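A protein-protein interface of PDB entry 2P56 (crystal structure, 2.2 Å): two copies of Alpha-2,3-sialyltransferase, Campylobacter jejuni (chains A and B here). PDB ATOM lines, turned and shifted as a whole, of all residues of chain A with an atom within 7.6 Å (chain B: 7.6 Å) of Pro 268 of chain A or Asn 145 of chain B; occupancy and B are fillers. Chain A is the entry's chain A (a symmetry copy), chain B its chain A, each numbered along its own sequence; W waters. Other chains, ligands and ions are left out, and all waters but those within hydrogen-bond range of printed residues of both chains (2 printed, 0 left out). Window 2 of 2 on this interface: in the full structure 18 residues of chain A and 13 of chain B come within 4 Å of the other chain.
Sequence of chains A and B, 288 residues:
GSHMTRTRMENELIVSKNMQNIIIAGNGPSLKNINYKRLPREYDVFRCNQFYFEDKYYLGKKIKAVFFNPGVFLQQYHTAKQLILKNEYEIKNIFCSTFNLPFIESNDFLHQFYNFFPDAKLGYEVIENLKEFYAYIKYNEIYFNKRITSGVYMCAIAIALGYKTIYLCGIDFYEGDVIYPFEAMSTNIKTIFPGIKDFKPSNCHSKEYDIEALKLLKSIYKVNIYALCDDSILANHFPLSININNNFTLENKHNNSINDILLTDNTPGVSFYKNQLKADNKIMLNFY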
ATOM      1  N   PHE A 116      -1.246   0.764  -8.236  1.00  0.00           N
ATOM      2  CA  PHE A 116      -1.694  -0.188  -7.226  1.00  0.00           C
ATOM      3  C   PHE A 116      -2.669   0.399  -6.218  1.00  0.00           C
ATOM      4  O   PHE A 116      -3.571  -0.294  -5.746  1.00  0.00           O
ATOM      5  CB  PHE A 116      -0.489  -0.741  -6.465  1.00  0.00           C
ATOM      6  CG  PHE A 116       0.218  -1.853  -7.175  1.00  0.00           C
ATOM      7  CD1 PHE A 116      -0.217  -3.171  -7.036  1.00  0.00           C
ATOM      8  CD2 PHE A 116       1.318  -1.591  -7.984  1.00  0.00           C
ATOM      9  CE1 PHE A 116       0.434  -4.213  -7.688  1.00  0.00           C
ATOM     10  CE2 PHE A 116       1.980  -2.627  -8.645  1.00  0.00           C
ATOM     11  CZ  PHE A 116       1.536  -3.940  -8.496  1.00  0.00           C
ATOM     12  N   ASP A 265      -2.836 -12.228   0.966  1.00  0.00           N
ATOM     13  CA  ASP A 265      -2.841 -13.534   0.307  1.00  0.00           C
ATOM     14  C   ASP A 265      -1.896 -13.470  -0.890  1.00  0.00           C
ATOM     15  O   ASP A 265      -1.751 -12.414  -1.516  1.00  0.00           O
ATOM     16  CB  ASP A 265      -4.252 -13.891  -0.173  1.00  0.00           C
ATOM     17  CG  ASP A 265      -5.096 -14.521   0.920  1.00  0.00           C
ATOM     18  OD1 ASP A 265      -6.340 -14.572   0.780  1.00  0.00           O
ATOM     19  OD2 ASP A 265      -4.506 -14.968   1.923  1.00  0.00           O
ATOM     20  N   ASN A 266      -1.266 -14.594  -1.216  1.00  0.00           N
ATOM     21  CA  ASN A 266      -0.330 -14.627  -2.334  1.00  0.00           C
ATOM     22  C   ASN A 266      -0.996 -14.716  -3.711  1.00  0.00           C
ATOM     23  O   ASN A 266      -0.772 -15.657  -4.473  1.00  0.00           O
ATOM     24  CB  ASN A 266       0.663 -15.775  -2.148  1.00  0.00           C
ATOM     25  CG  ASN A 266       1.844 -15.681  -3.091  1.00  0.00           C
ATOM     26  OD1 ASN A 266       1.947 -16.442  -4.055  1.00  0.00           O
ATOM     27  ND2 ASN A 266       2.741 -14.734  -2.823  1.00  0.00           N
ATOM     28  N   THR A 267      -1.823 -13.723  -4.012  1.00  0.00           N
ATOM     29  CA  THR A 267      -2.514 -13.628  -5.290  1.00  0.00           C
ATOM     30  C   THR A 267      -1.458 -13.261  -6.331  1.00  0.00           C
ATOM     31  O   THR A 267      -0.306 -13.007  -5.989  1.00  0.00           O
ATOM     32  CB  THR A 267      -3.560 -12.496  -5.272  1.00  0.00           C
ATOM     33  OG1 THR A 267      -2.898 -11.257  -4.988  1.00  0.00           O
ATOM     34  CG2 THR A 267      -4.627 -12.749  -4.208  1.00  0.00           C
ATOM     35  N   PRO A 268      -1.832 -13.249  -7.620  1.00  0.00           N
ATOM     36  CA  PRO A 268      -0.846 -12.890  -8.652  1.00  0.00           C
ATOM     37  C   PRO A 268      -0.369 -11.441  -8.466  1.00  0.00           C
ATOM     38  O   PRO A 268       0.808 -11.135  -8.664  1.00  0.00           O
ATOM     39  CB  PRO A 268      -1.618 -13.087  -9.956  1.00  0.00           C
ATOM     40  CG  PRO A 268      -2.548 -14.233  -9.615  1.00  0.00           C
ATOM     41  CD  PRO A 268      -3.031 -13.866  -8.218  1.00  0.00           C
ATOM     42  N   GLY A 269      -1.291 -10.561  -8.067  1.00  0.00           N
ATOM     43  CA  GLY A 269      -0.954  -9.162  -7.852  1.00  0.00           C
ATOM     44  C   GLY A 269      -0.029  -8.944  -6.667  1.00  0.00           C
ATOM     45  O   GLY A 269       0.944  -8.195  -6.758  1.00  0.00           O
ATOM     46  N   VAL A 270      -0.334  -9.595  -5.548  1.00  0.00           N
ATOM     47  CA  VAL A 270       0.487  -9.470  -4.351  1.00  0.00           C
ATOM     48  C   VAL A 270       1.863 -10.097  -4.552  1.00  0.00           C
ATOM     49  O   VAL A 270       2.876  -9.518  -4.152  1.00  0.00           O
ATOM     50  CB  VAL A 270      -0.194 -10.133  -3.124  1.00  0.00           C
ATOM     51  CG1 VAL A 270       0.826 -10.358  -2.001  1.00  0.00           C
ATOM     52  CG2 VAL A 270      -1.323  -9.245  -2.618  1.00  0.00           C
ATOM     53  N   SER A 271       1.914 -11.276  -5.170  1.00  0.00           N
ATOM     54  CA  SER A 271       3.209 -11.923  -5.387  1.00  0.00           C
ATOM     55  C   SER A 271       4.071 -11.071  -6.322  1.00  0.00           C
ATOM     56  O   SER A 271       5.283 -10.962  -6.127  1.00  0.00           O
ATOM     57  CB  SER A 271       3.031 -13.351  -5.937  1.00  0.00           C
ATOM     58  OG  SER A 271       2.266 -13.363  -7.125  1.00  0.00           O
ATOM     59  N   PHE A 272       3.449 -10.455  -7.325  1.00  0.00           N
ATOM     60  CA  PHE A 272       4.187  -9.587  -8.239  1.00  0.00           C
ATOM     61  C   PHE A 272       4.762  -8.395  -7.462  1.00  0.00           C
ATOM     62  O   PHE A 272       5.941  -8.054  -7.603  1.00  0.00           O
ATOM     63  CB  PHE A 272       3.271  -9.074  -9.366  1.00  0.00           C
ATOM     64  CG  PHE A 272       3.909  -8.004 -10.225  1.00  0.00           C
ATOM     65  CD1 PHE A 272       3.913  -6.669  -9.818  1.00  0.00           C
ATOM     66  CD2 PHE A 272       4.567  -8.343 -11.404  1.00  0.00           C
ATOM     67  CE1 PHE A 272       4.567  -5.694 -10.569  1.00  0.00           C
ATOM     68  CE2 PHE A 272       5.226  -7.375 -12.162  1.00  0.00           C
ATOM     69  CZ  PHE A 272       5.229  -6.049 -11.745  1.00  0.00           C
ATOM     70  N   TYR A 273       3.918  -7.775  -6.639  1.00  0.00           N
ATOM     71  CA  TYR A 273       4.305  -6.617  -5.828  1.00  0.00           C
ATOM     72  C   TYR A 273       5.450  -6.943  -4.866  1.00  0.00           C
ATOM     73  O   TYR A 273       6.453  -6.235  -4.821  1.00  0.00           O
ATOM     74  CB  TYR A 273       3.097  -6.122  -5.019  1.00  0.00           C
ATOM     75  CG  TYR A 273       3.322  -4.819  -4.279  1.00  0.00           C
ATOM     76  CD1 TYR A 273       2.940  -3.595  -4.840  1.00  0.00           C
ATOM     77  CD2 TYR A 273       3.911  -4.809  -3.014  1.00  0.00           C
ATOM     78  CE1 TYR A 273       3.138  -2.387  -4.151  1.00  0.00           C
ATOM     79  CE2 TYR A 273       4.114  -3.613  -2.323  1.00  0.00           C
ATOM     80  CZ  TYR A 273       3.727  -2.413  -2.891  1.00  0.00           C
ATOM     81  OH  TYR A 273       3.930  -1.247  -2.192  1.00  0.00           O
ATOM     82  N   LYS A 274       5.283  -8.010  -4.088  1.00  0.00           N
ATOM     83  CA  LYS A 274       6.297  -8.427  -3.129  1.00  0.00           C
ATOM     84  C   LYS A 274       7.594  -8.858  -3.806  1.00  0.00           C
ATOM     85  O   LYS A 274       8.681  -8.599  -3.300  1.00  0.00           O
ATOM     86  CB  LYS A 274       5.782  -9.589  -2.273  1.00  0.00           C
ATOM     87  CG  LYS A 274       4.764  -9.206  -1.223  1.00  0.00           C
ATOM     88  CD  LYS A 274       4.381 -10.411  -0.359  1.00  0.00           C
ATOM     89  CE  LYS A 274       3.308 -10.051   0.666  1.00  0.00           C
ATOM     90  NZ  LYS A 274       2.888 -11.220   1.492  1.00  0.00           N
ATOM     91  N   PHE B 103       1.017  -6.368 -13.501  1.00  0.00           N
ATOM     92  CA  PHE B 103       0.988  -7.827 -13.572  1.00  0.00           C
ATOM     93  C   PHE B 103      -0.085  -8.303 -14.556  1.00  0.00           C
ATOM     94  O   PHE B 103      -0.303  -9.501 -14.712  1.00  0.00           O
ATOM     95  CB  PHE B 103       0.768  -8.458 -12.183  1.00  0.00           C
ATOM     96  CG  PHE B 103      -0.445  -7.945 -11.465  1.00  0.00           C
ATOM     97  CD1 PHE B 103      -0.388  -6.761 -10.732  1.00  0.00           C
ATOM     98  CD2 PHE B 103      -1.652  -8.642 -11.528  1.00  0.00           C
ATOM     99  CE1 PHE B 103      -1.520  -6.275 -10.066  1.00  0.00           C
ATOM    100  CE2 PHE B 103      -2.788  -8.170 -10.871  1.00  0.00           C
ATOM    101  CZ  PHE B 103      -2.724  -6.981 -10.135  1.00  0.00           C
ATOM    102  N   ILE B 104      -0.756  -7.358 -15.215  1.00  0.00           N
ATOM    103  CA  ILE B 104      -1.772  -7.694 -16.215  1.00  0.00           C
ATOM    104  C   ILE B 104      -1.289  -7.172 -17.570  1.00  0.00           C
ATOM    105  O   ILE B 104      -1.313  -7.890 -18.564  1.00  0.00           O
ATOM    106  CB  ILE B 104      -3.150  -7.055 -15.901  1.00  0.00           C
ATOM    107  CG1 ILE B 104      -3.646  -7.505 -14.520  1.00  0.00           C
ATOM    108  CG2 ILE B 104      -4.161  -7.451 -16.989  1.00  0.00           C
ATOM    109  CD1 ILE B 104      -5.020  -6.940 -14.138  1.00  0.00           C
ATOM    110  N   ILE B 137     -12.295  -2.050  -7.953  1.00  0.00           N
ATOM    111  CA  ILE B 137     -11.879  -3.217  -8.731  1.00  0.00           C
ATOM    112  C   ILE B 137     -10.393  -3.518  -8.561  1.00  0.00           C
ATOM    113  O   ILE B 137      -9.997  -4.681  -8.586  1.00  0.00           O
ATOM    114  CB  ILE B 137     -12.236  -3.100 -10.250  1.00  0.00           C
ATOM    115  CG1 ILE B 137     -11.491  -1.941 -10.909  1.00  0.00           C
ATOM    116  CG2 ILE B 137     -13.752  -2.908 -10.409  1.00  0.00           C
ATOM    117  CD1 ILE B 137     -11.820  -1.793 -12.387  1.00  0.00           C
ATOM    118  N   LYS B 138      -9.568  -2.488  -8.362  1.00  0.00           N
ATOM    119  CA  LYS B 138      -8.137  -2.726  -8.171  1.00  0.00           C
ATOM    120  C   LYS B 138      -7.883  -3.411  -6.831  1.00  0.00           C
ATOM    121  O   LYS B 138      -7.001  -4.269  -6.711  1.00  0.00           O
ATOM    122  CB  LYS B 138      -7.335  -1.414  -8.265  1.00  0.00           C
ATOM    123  CG  LYS B 138      -7.369  -0.814  -9.677  1.00  0.00           C
ATOM    124  CD  LYS B 138      -6.126  -0.009 -10.001  1.00  0.00           C
ATOM    125  CE  LYS B 138      -5.933   0.085 -11.510  1.00  0.00           C
ATOM    126  NZ  LYS B 138      -4.662   0.771 -11.871  1.00  0.00           N
ATOM    127  N   TYR B 139      -8.665  -3.038  -5.822  1.00  0.00           N
ATOM    128  CA  TYR B 139      -8.514  -3.641  -4.508  1.00  0.00           C
ATOM    129  C   TYR B 139      -8.864  -5.131  -4.620  1.00  0.00           C
ATOM    130  O   TYR B 139      -8.114  -5.997  -4.168  1.00  0.00           O
ATOM    131  CB  TYR B 139      -9.430  -2.943  -3.494  1.00  0.00           C
ATOM    132  CG  TYR B 139      -9.332  -3.499  -2.087  1.00  0.00           C
ATOM    133  CD1 TYR B 139      -8.115  -3.520  -1.404  1.00  0.00           C
ATOM    134  CD2 TYR B 139     -10.453  -4.035  -1.452  1.00  0.00           C
ATOM    135  CE1 TYR B 139      -8.014  -4.064  -0.131  1.00  0.00           C
ATOM    136  CE2 TYR B 139     -10.368  -4.581  -0.170  1.00  0.00           C
ATOM    137  CZ  TYR B 139      -9.152  -4.595   0.483  1.00  0.00           C
ATOM    138  OH  TYR B 139      -9.080  -5.133   1.748  1.00  0.00           O
ATOM    139  N   ASN B 140      -9.993  -5.431  -5.249  1.00  0.00           N
ATOM    140  CA  ASN B 140     -10.405  -6.823  -5.399  1.00  0.00           C
ATOM    141  C   ASN B 140      -9.448  -7.633  -6.255  1.00  0.00           C
ATOM    142  O   ASN B 140      -9.135  -8.772  -5.926  1.00  0.00           O
ATOM    143  CB  ASN B 140     -11.817  -6.894  -5.971  1.00  0.00           C
ATOM    144  CG  ASN B 140     -12.864  -6.604  -4.928  1.00  0.00           C
ATOM    145  OD1 ASN B 140     -13.088  -7.407  -4.029  1.00  0.00           O
ATOM    146  ND2 ASN B 140     -13.502  -5.448  -5.028  1.00  0.00           N
ATOM    147  N   GLU B 141      -8.975  -7.039  -7.347  1.00  0.00           N
ATOM    148  CA  GLU B 141      -8.034  -7.714  -8.230  1.00  0.00           C
ATOM    149  C   GLU B 141      -6.755  -8.057  -7.484  1.00  0.00           C
ATOM    150  O   GLU B 141      -6.389  -9.223  -7.337  1.00  0.00           O
ATOM    151  CB  GLU B 141      -7.690  -6.810  -9.421  1.00  0.00           C
ATOM    152  CG  GLU B 141      -6.548  -7.305 -10.320  1.00  0.00           C
ATOM    153  CD  GLU B 141      -6.961  -8.430 -11.271  1.00  0.00           C
ATOM    154  OE1 GLU B 141      -8.062  -8.350 -11.856  1.00  0.00           O
ATOM    155  OE2 GLU B 141      -6.173  -9.386 -11.449  1.00  0.00           O
ATOM    156  N   ILE B 142      -6.082  -7.023  -7.002  1.00  0.00           N
ATOM    157  CA  ILE B 142      -4.816  -7.185  -6.305  1.00  0.00           C
ATOM    158  C   ILE B 142      -4.817  -8.053  -5.057  1.00  0.00           C
ATOM    159  O   ILE B 142      -3.978  -8.949  -4.910  1.00  0.00           O
ATOM    160  CB  ILE B 142      -4.227  -5.805  -5.933  1.00  0.00           C
ATOM    161  CG1 ILE B 142      -3.931  -5.019  -7.217  1.00  0.00           C
ATOM    162  CG2 ILE B 142      -2.954  -5.975  -5.097  1.00  0.00           C
ATOM    163  CD1 ILE B 142      -3.643  -3.559  -6.989  1.00  0.00           C
ATOM    164  N   TYR B 143      -5.749  -7.801  -4.150  1.00  0.00           N
ATOM    165  CA  TYR B 143      -5.760  -8.560  -2.907  1.00  0.00           C
ATOM    166  C   TYR B 143      -6.619  -9.822  -2.874  1.00  0.00           C
ATOM    167  O   TYR B 143      -6.428 -10.672  -2.005  1.00  0.00           O
ATOM    168  CB  TYR B 143      -6.172  -7.639  -1.756  1.00  0.00           C
ATOM    169  CG  TYR B 143      -5.200  -6.510  -1.478  1.00  0.00           C
ATOM    170  CD1 TYR B 143      -4.175  -6.653  -0.538  1.00  0.00           C
ATOM    171  CD2 TYR B 143      -5.314  -5.291  -2.145  1.00  0.00           C
ATOM    172  CE1 TYR B 143      -3.290  -5.599  -0.266  1.00  0.00           C
ATOM    173  CE2 TYR B 143      -4.434  -4.230  -1.884  1.00  0.00           C
ATOM    174  CZ  TYR B 143      -3.431  -4.388  -0.945  1.00  0.00           C
ATOM    175  OH  TYR B 143      -2.594  -3.329  -0.665  1.00  0.00           O
ATOM    176  N   PHE B 144      -7.548  -9.962  -3.811  1.00  0.00           N
ATOM    177  CA  PHE B 144      -8.431 -11.126  -3.797  1.00  0.00           C
ATOM    178  C   PHE B 144      -8.518 -11.897  -5.110  1.00  0.00           C
ATOM    179  O   PHE B 144      -9.263 -12.872  -5.200  1.00  0.00           O
ATOM    180  CB  PHE B 144      -9.837 -10.686  -3.369  1.00  0.00           C
ATOM    181  CG  PHE B 144      -9.883 -10.066  -2.008  1.00  0.00           C
ATOM    182  CD1 PHE B 144      -9.780 -10.854  -0.868  1.00  0.00           C
ATOM    183  CD2 PHE B 144      -9.983  -8.688  -1.862  1.00  0.00           C
ATOM    184  CE1 PHE B 144      -9.775 -10.280   0.396  1.00  0.00           C
ATOM    185  CE2 PHE B 144      -9.978  -8.099  -0.598  1.00  0.00           C
ATOM    186  CZ  PHE B 144      -9.873  -8.892   0.532  1.00  0.00           C
ATOM    187  N   ASN B 145      -7.774 -11.460  -6.125  1.00  0.00           N
ATOM    188  CA  ASN B 145      -7.778 -12.128  -7.427  1.00  0.00           C
ATOM    189  C   ASN B 145      -9.171 -12.185  -8.064  1.00  0.00           C
ATOM    190  O   ASN B 145      -9.571 -13.210  -8.611  1.00  0.00           O
ATOM    191  CB  ASN B 145      -7.231 -13.556  -7.289  1.00  0.00           C
ATOM    192  CG  ASN B 145      -6.909 -14.199  -8.635  1.00  0.00           C
ATOM    193  OD1 ASN B 145      -6.798 -15.420  -8.733  1.00  0.00           O
ATOM    194  ND2 ASN B 145      -6.744 -13.378  -9.669  1.00  0.00           N
ATOM    195  N   LYS B 146      -9.924 -11.096  -7.974  1.00  0.00           N
ATOM    196  CA  LYS B 146     -11.244 -11.056  -8.596  1.00  0.00           C
ATOM    197  C   LYS B 146     -11.194 -10.006  -9.697  1.00  0.00           C
ATOM    198  O   LYS B 146     -10.740  -8.878  -9.485  1.00  0.00           O
ATOM    199  CB  LYS B 146     -12.337 -10.712  -7.572  1.00  0.00           C
ATOM    200  CG  LYS B 146     -12.539 -11.796  -6.515  1.00  0.00           C
ATOM    201  CD  LYS B 146     -13.865 -11.646  -5.780  1.00  0.00           C
ATOM    202  CE  LYS B 146     -14.008 -10.279  -5.127  1.00  0.00           C
ATOM    203  NZ  LYS B 146     -15.285 -10.169  -4.355  1.00  0.00           N
ATOM    204  N   ARG B 147     -11.651 -10.382 -10.882  1.00  0.00           N
ATOM    205  CA  ARG B 147     -11.627  -9.468 -12.012  1.00  0.00           C
ATOM    206  C   ARG B 147     -12.977  -9.476 -12.704  1.00  0.00           C
ATOM    207  O   ARG B 147     -13.613 -10.522 -12.819  1.00  0.00           O
ATOM    208  CB  ARG B 147     -10.529  -9.906 -12.988  1.00  0.00           C
ATOM    209  CG  ARG B 147     -10.393  -9.056 -14.233  1.00  0.00           C
ATOM    210  CD  ARG B 147      -9.263  -9.575 -15.090  1.00  0.00           C
ATOM    211  NE  ARG B 147      -8.016  -9.677 -14.334  1.00  0.00           N
ATOM    212  CZ  ARG B 147      -6.883 -10.166 -14.829  1.00  0.00           C
ATOM    213  NH1 ARG B 147      -6.843 -10.597 -16.083  1.00  0.00           N
ATOM    214  NH2 ARG B 147      -5.793 -10.233 -14.074  1.00  0.00           N
ATOM    215  N   ASN B 203      -9.997 -18.234 -13.233  1.00  0.00           N
ATOM    216  CA  ASN B 203     -10.462 -18.402 -11.862  1.00  0.00           C
ATOM    217  C   ASN B 203     -10.642 -17.068 -11.133  1.00  0.00           C
ATOM    218  O   ASN B 203     -10.948 -17.046  -9.939  1.00  0.00           O
ATOM    219  CB  ASN B 203      -9.482 -19.276 -11.075  1.00  0.00           C
ATOM    220  CG  ASN B 203      -8.143 -18.598 -10.852  1.00  0.00           C
ATOM    221  OD1 ASN B 203      -7.291 -19.105 -10.120  1.00  0.00           O
ATOM    222  ND2 ASN B 203      -7.948 -17.444 -11.483  1.00  0.00           N
ATOM    223  N   CYS B 204     -10.440 -15.960 -11.840  1.00  0.00           N
ATOM    224  CA  CYS B 204     -10.598 -14.641 -11.230  1.00  0.00           C
ATOM    225  C   CYS B 204     -11.968 -14.045 -11.548  1.00  0.00           C
ATOM    226  O   CYS B 204     -12.378 -13.052 -10.951  1.00  0.00           O
ATOM    227  CB  CYS B 204      -9.483 -13.694 -11.694  1.00  0.00           C
ATOM    228  SG  CYS B 204      -9.315 -13.480 -13.490  1.00  0.00           S
ATOM    229  N   HIS B 205     -12.675 -14.664 -12.492  1.00  0.00           N
ATOM    230  CA  HIS B 205     -14.004 -14.205 -12.880  1.00  0.00           C
ATOM    231  C   HIS B 205     -15.077 -15.037 -12.188  1.00  0.00           C
ATOM    232  O   HIS B 205     -14.866 -16.214 -11.895  1.00  0.00           O
ATOM    233  CB  HIS B 205     -14.195 -14.317 -14.395  1.00  0.00           C
ATOM    234  CG  HIS B 205     -13.282 -13.441 -15.192  1.00  0.00           C
ATOM    235  ND1 HIS B 205     -12.232 -13.937 -15.935  1.00  0.00           N
ATOM    236  CD2 HIS B 205     -13.269 -12.100 -15.374  1.00  0.00           C
ATOM    237  CE1 HIS B 205     -11.613 -12.939 -16.540  1.00  0.00           C
ATOM    238  NE2 HIS B 205     -12.222 -11.814 -16.216  1.00  0.00           N
ATOM    239  N   SER B 206     -16.227 -14.426 -11.925  1.00  0.00           N
ATOM    240  CA  SER B 206     -17.320 -15.149 -11.283  1.00  0.00           C
ATOM    241  C   SER B 206     -18.638 -14.424 -11.477  1.00  0.00           C
ATOM    242  O   SER B 206     -18.686 -13.194 -11.582  1.00  0.00           O
ATOM    243  CB  SER B 206     -17.059 -15.331  -9.784  1.00  0.00           C
ATOM    244  OG  SER B 206     -17.301 -14.128  -9.072  1.00  0.00           O
ATOM    245  N   TYR B 209     -19.175 -11.923  -8.587  1.00  0.00           N
ATOM    246  CA  TYR B 209     -18.407 -10.687  -8.618  1.00  0.00           C
ATOM    247  C   TYR B 209     -18.987  -9.767  -9.681  1.00  0.00           C
ATOM    248  O   TYR B 209     -19.175  -8.568  -9.444  1.00  0.00           O
ATOM    249  CB  TYR B 209     -16.919 -10.952  -8.885  1.00  0.00           C
ATOM    250  CG  TYR B 209     -16.069  -9.705  -8.721  1.00  0.00           C
ATOM    251  CD1 TYR B 209     -16.238  -8.873  -7.611  1.00  0.00           C
ATOM    252  CD2 TYR B 209     -15.144  -9.324  -9.696  1.00  0.00           C
ATOM    253  CE1 TYR B 209     -15.518  -7.687  -7.479  1.00  0.00           C
ATOM    254  CE2 TYR B 209     -14.411  -8.136  -9.574  1.00  0.00           C
ATOM    255  CZ  TYR B 209     -14.610  -7.322  -8.464  1.00  0.00           C
ATOM    256  OH  TYR B 209     -13.930  -6.133  -8.345  1.00  0.00           O
HETATM  257  O   HOH W   1      -4.099 -10.625  -7.966  1.00  0.00           O
HETATM  258  O   HOH W   2      -5.749  -1.910  -4.359  1.00  0.00           O
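The side-chain hydroxyl of Thr 267 of chain A sits at hydrogen-bond distance from the backbone carbonyl oxygen of Ile 142 of chain B (2.5 Å).
The backbone NH (N) of Val 270 of chain A is in hydrogen-bond range of the side-chain hydroxyl (OG1) of Thr 267 of chain A, 3.1 Å away. The backbone carbonyl oxygen (O) of Thr 267 of chain A lies within hydrogen-bond range of the side-chain hydroxyl (OG) of Ser 271 of chain A (2.8 Å). The backbone carbonyl oxygen of Asn 140 of chain B sits at hydrogen-bond distance from the backbone NH of Asn 145 of chain B, at 3.0 Å. The backbone carbonyl oxygen (O) of Pro 268 of chain A lies within hydrogen-bond range of the side-chain hydroxyl (OG) of Ser 271 of chain A.
Phe 103 of chain B touches Phe 116 of chain A (CE1 to CE1, 3.7 Å). CD1 of Phe 116 of chain A touches CD1 of Ile 142 of chain B, at 3.4 Å. CG2 of Thr 267 of chain A touches O of Tyr 143 of chain B, 3.5 Å away. Thr 267 of chain A touches Asn 145 of chain B. CG of Asn 145 of chain B touches CD of Pro 268 of chain A, 3.9 Å away. Gly 269 of chain A touches Phe 103 of chain B. Val 270 of chain A touches Ile 142 of chain B (CG2 to O, 3.5 Å). Phe 103 of chain B touches Phe 272 of chain A (CB to CG, 3.7 Å).
Of chain A, only Thr 267 (3.9 Å) and Pro 268 (3.9 Å) come within 4 Å of Asn 145 of chain B. Of chain B, only Phe 103 comes within 4 Å of Gly 269 of chain A. Of the printed residues of chain B, Thr 267 of chain A touches Ile 142 (2.5 Å), Tyr 143 (3.5 Å) and Asn 145 (3.9 Å). Printed residues of chain A within 4 Å of Tyr 143 of chain B: Thr 267. Of the printed residues of chain B, Phe 116 of chain A touches Phe 103 (3.7 Å) and Ile 142 (3.4 Å). Tyr 139 of chain B touches none of the printed residues of chain A. Arg 147 of chain B touches none of the printed residues of chain A.
Printed residues of chain A that touch a printed residue of chain B: Phe 116, Thr 267, Pro 268, Gly 269, Val 270 and Phe 272. Among the printed residues, no Asp or Glu carboxylate lies within 4 Å of a Lys or Arg side-chain nitrogen of the other chain.
No position is printed for both chains. Of the 9 pairs that touch across the chains among the printed residues, none has its exchanged pair printed and touching as well.
Water W1 lies within hydrogen-bond range of the backbone carbonyl oxygen (O) of Glu 141 of chain B, the backbone NH (N) of Gly 269 of chain A, the side-chain hydroxyl (OG1) of Thr 267 of chain A and the backbone carbonyl oxygen (O) of Ile 142 of chain B. Water W2 bridges the backbone carbonyl oxygen (O) of Phe 116 of chain A (3.0 Å) and the backbone NH (N) of Tyr 139 of chain B (3.5 Å).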
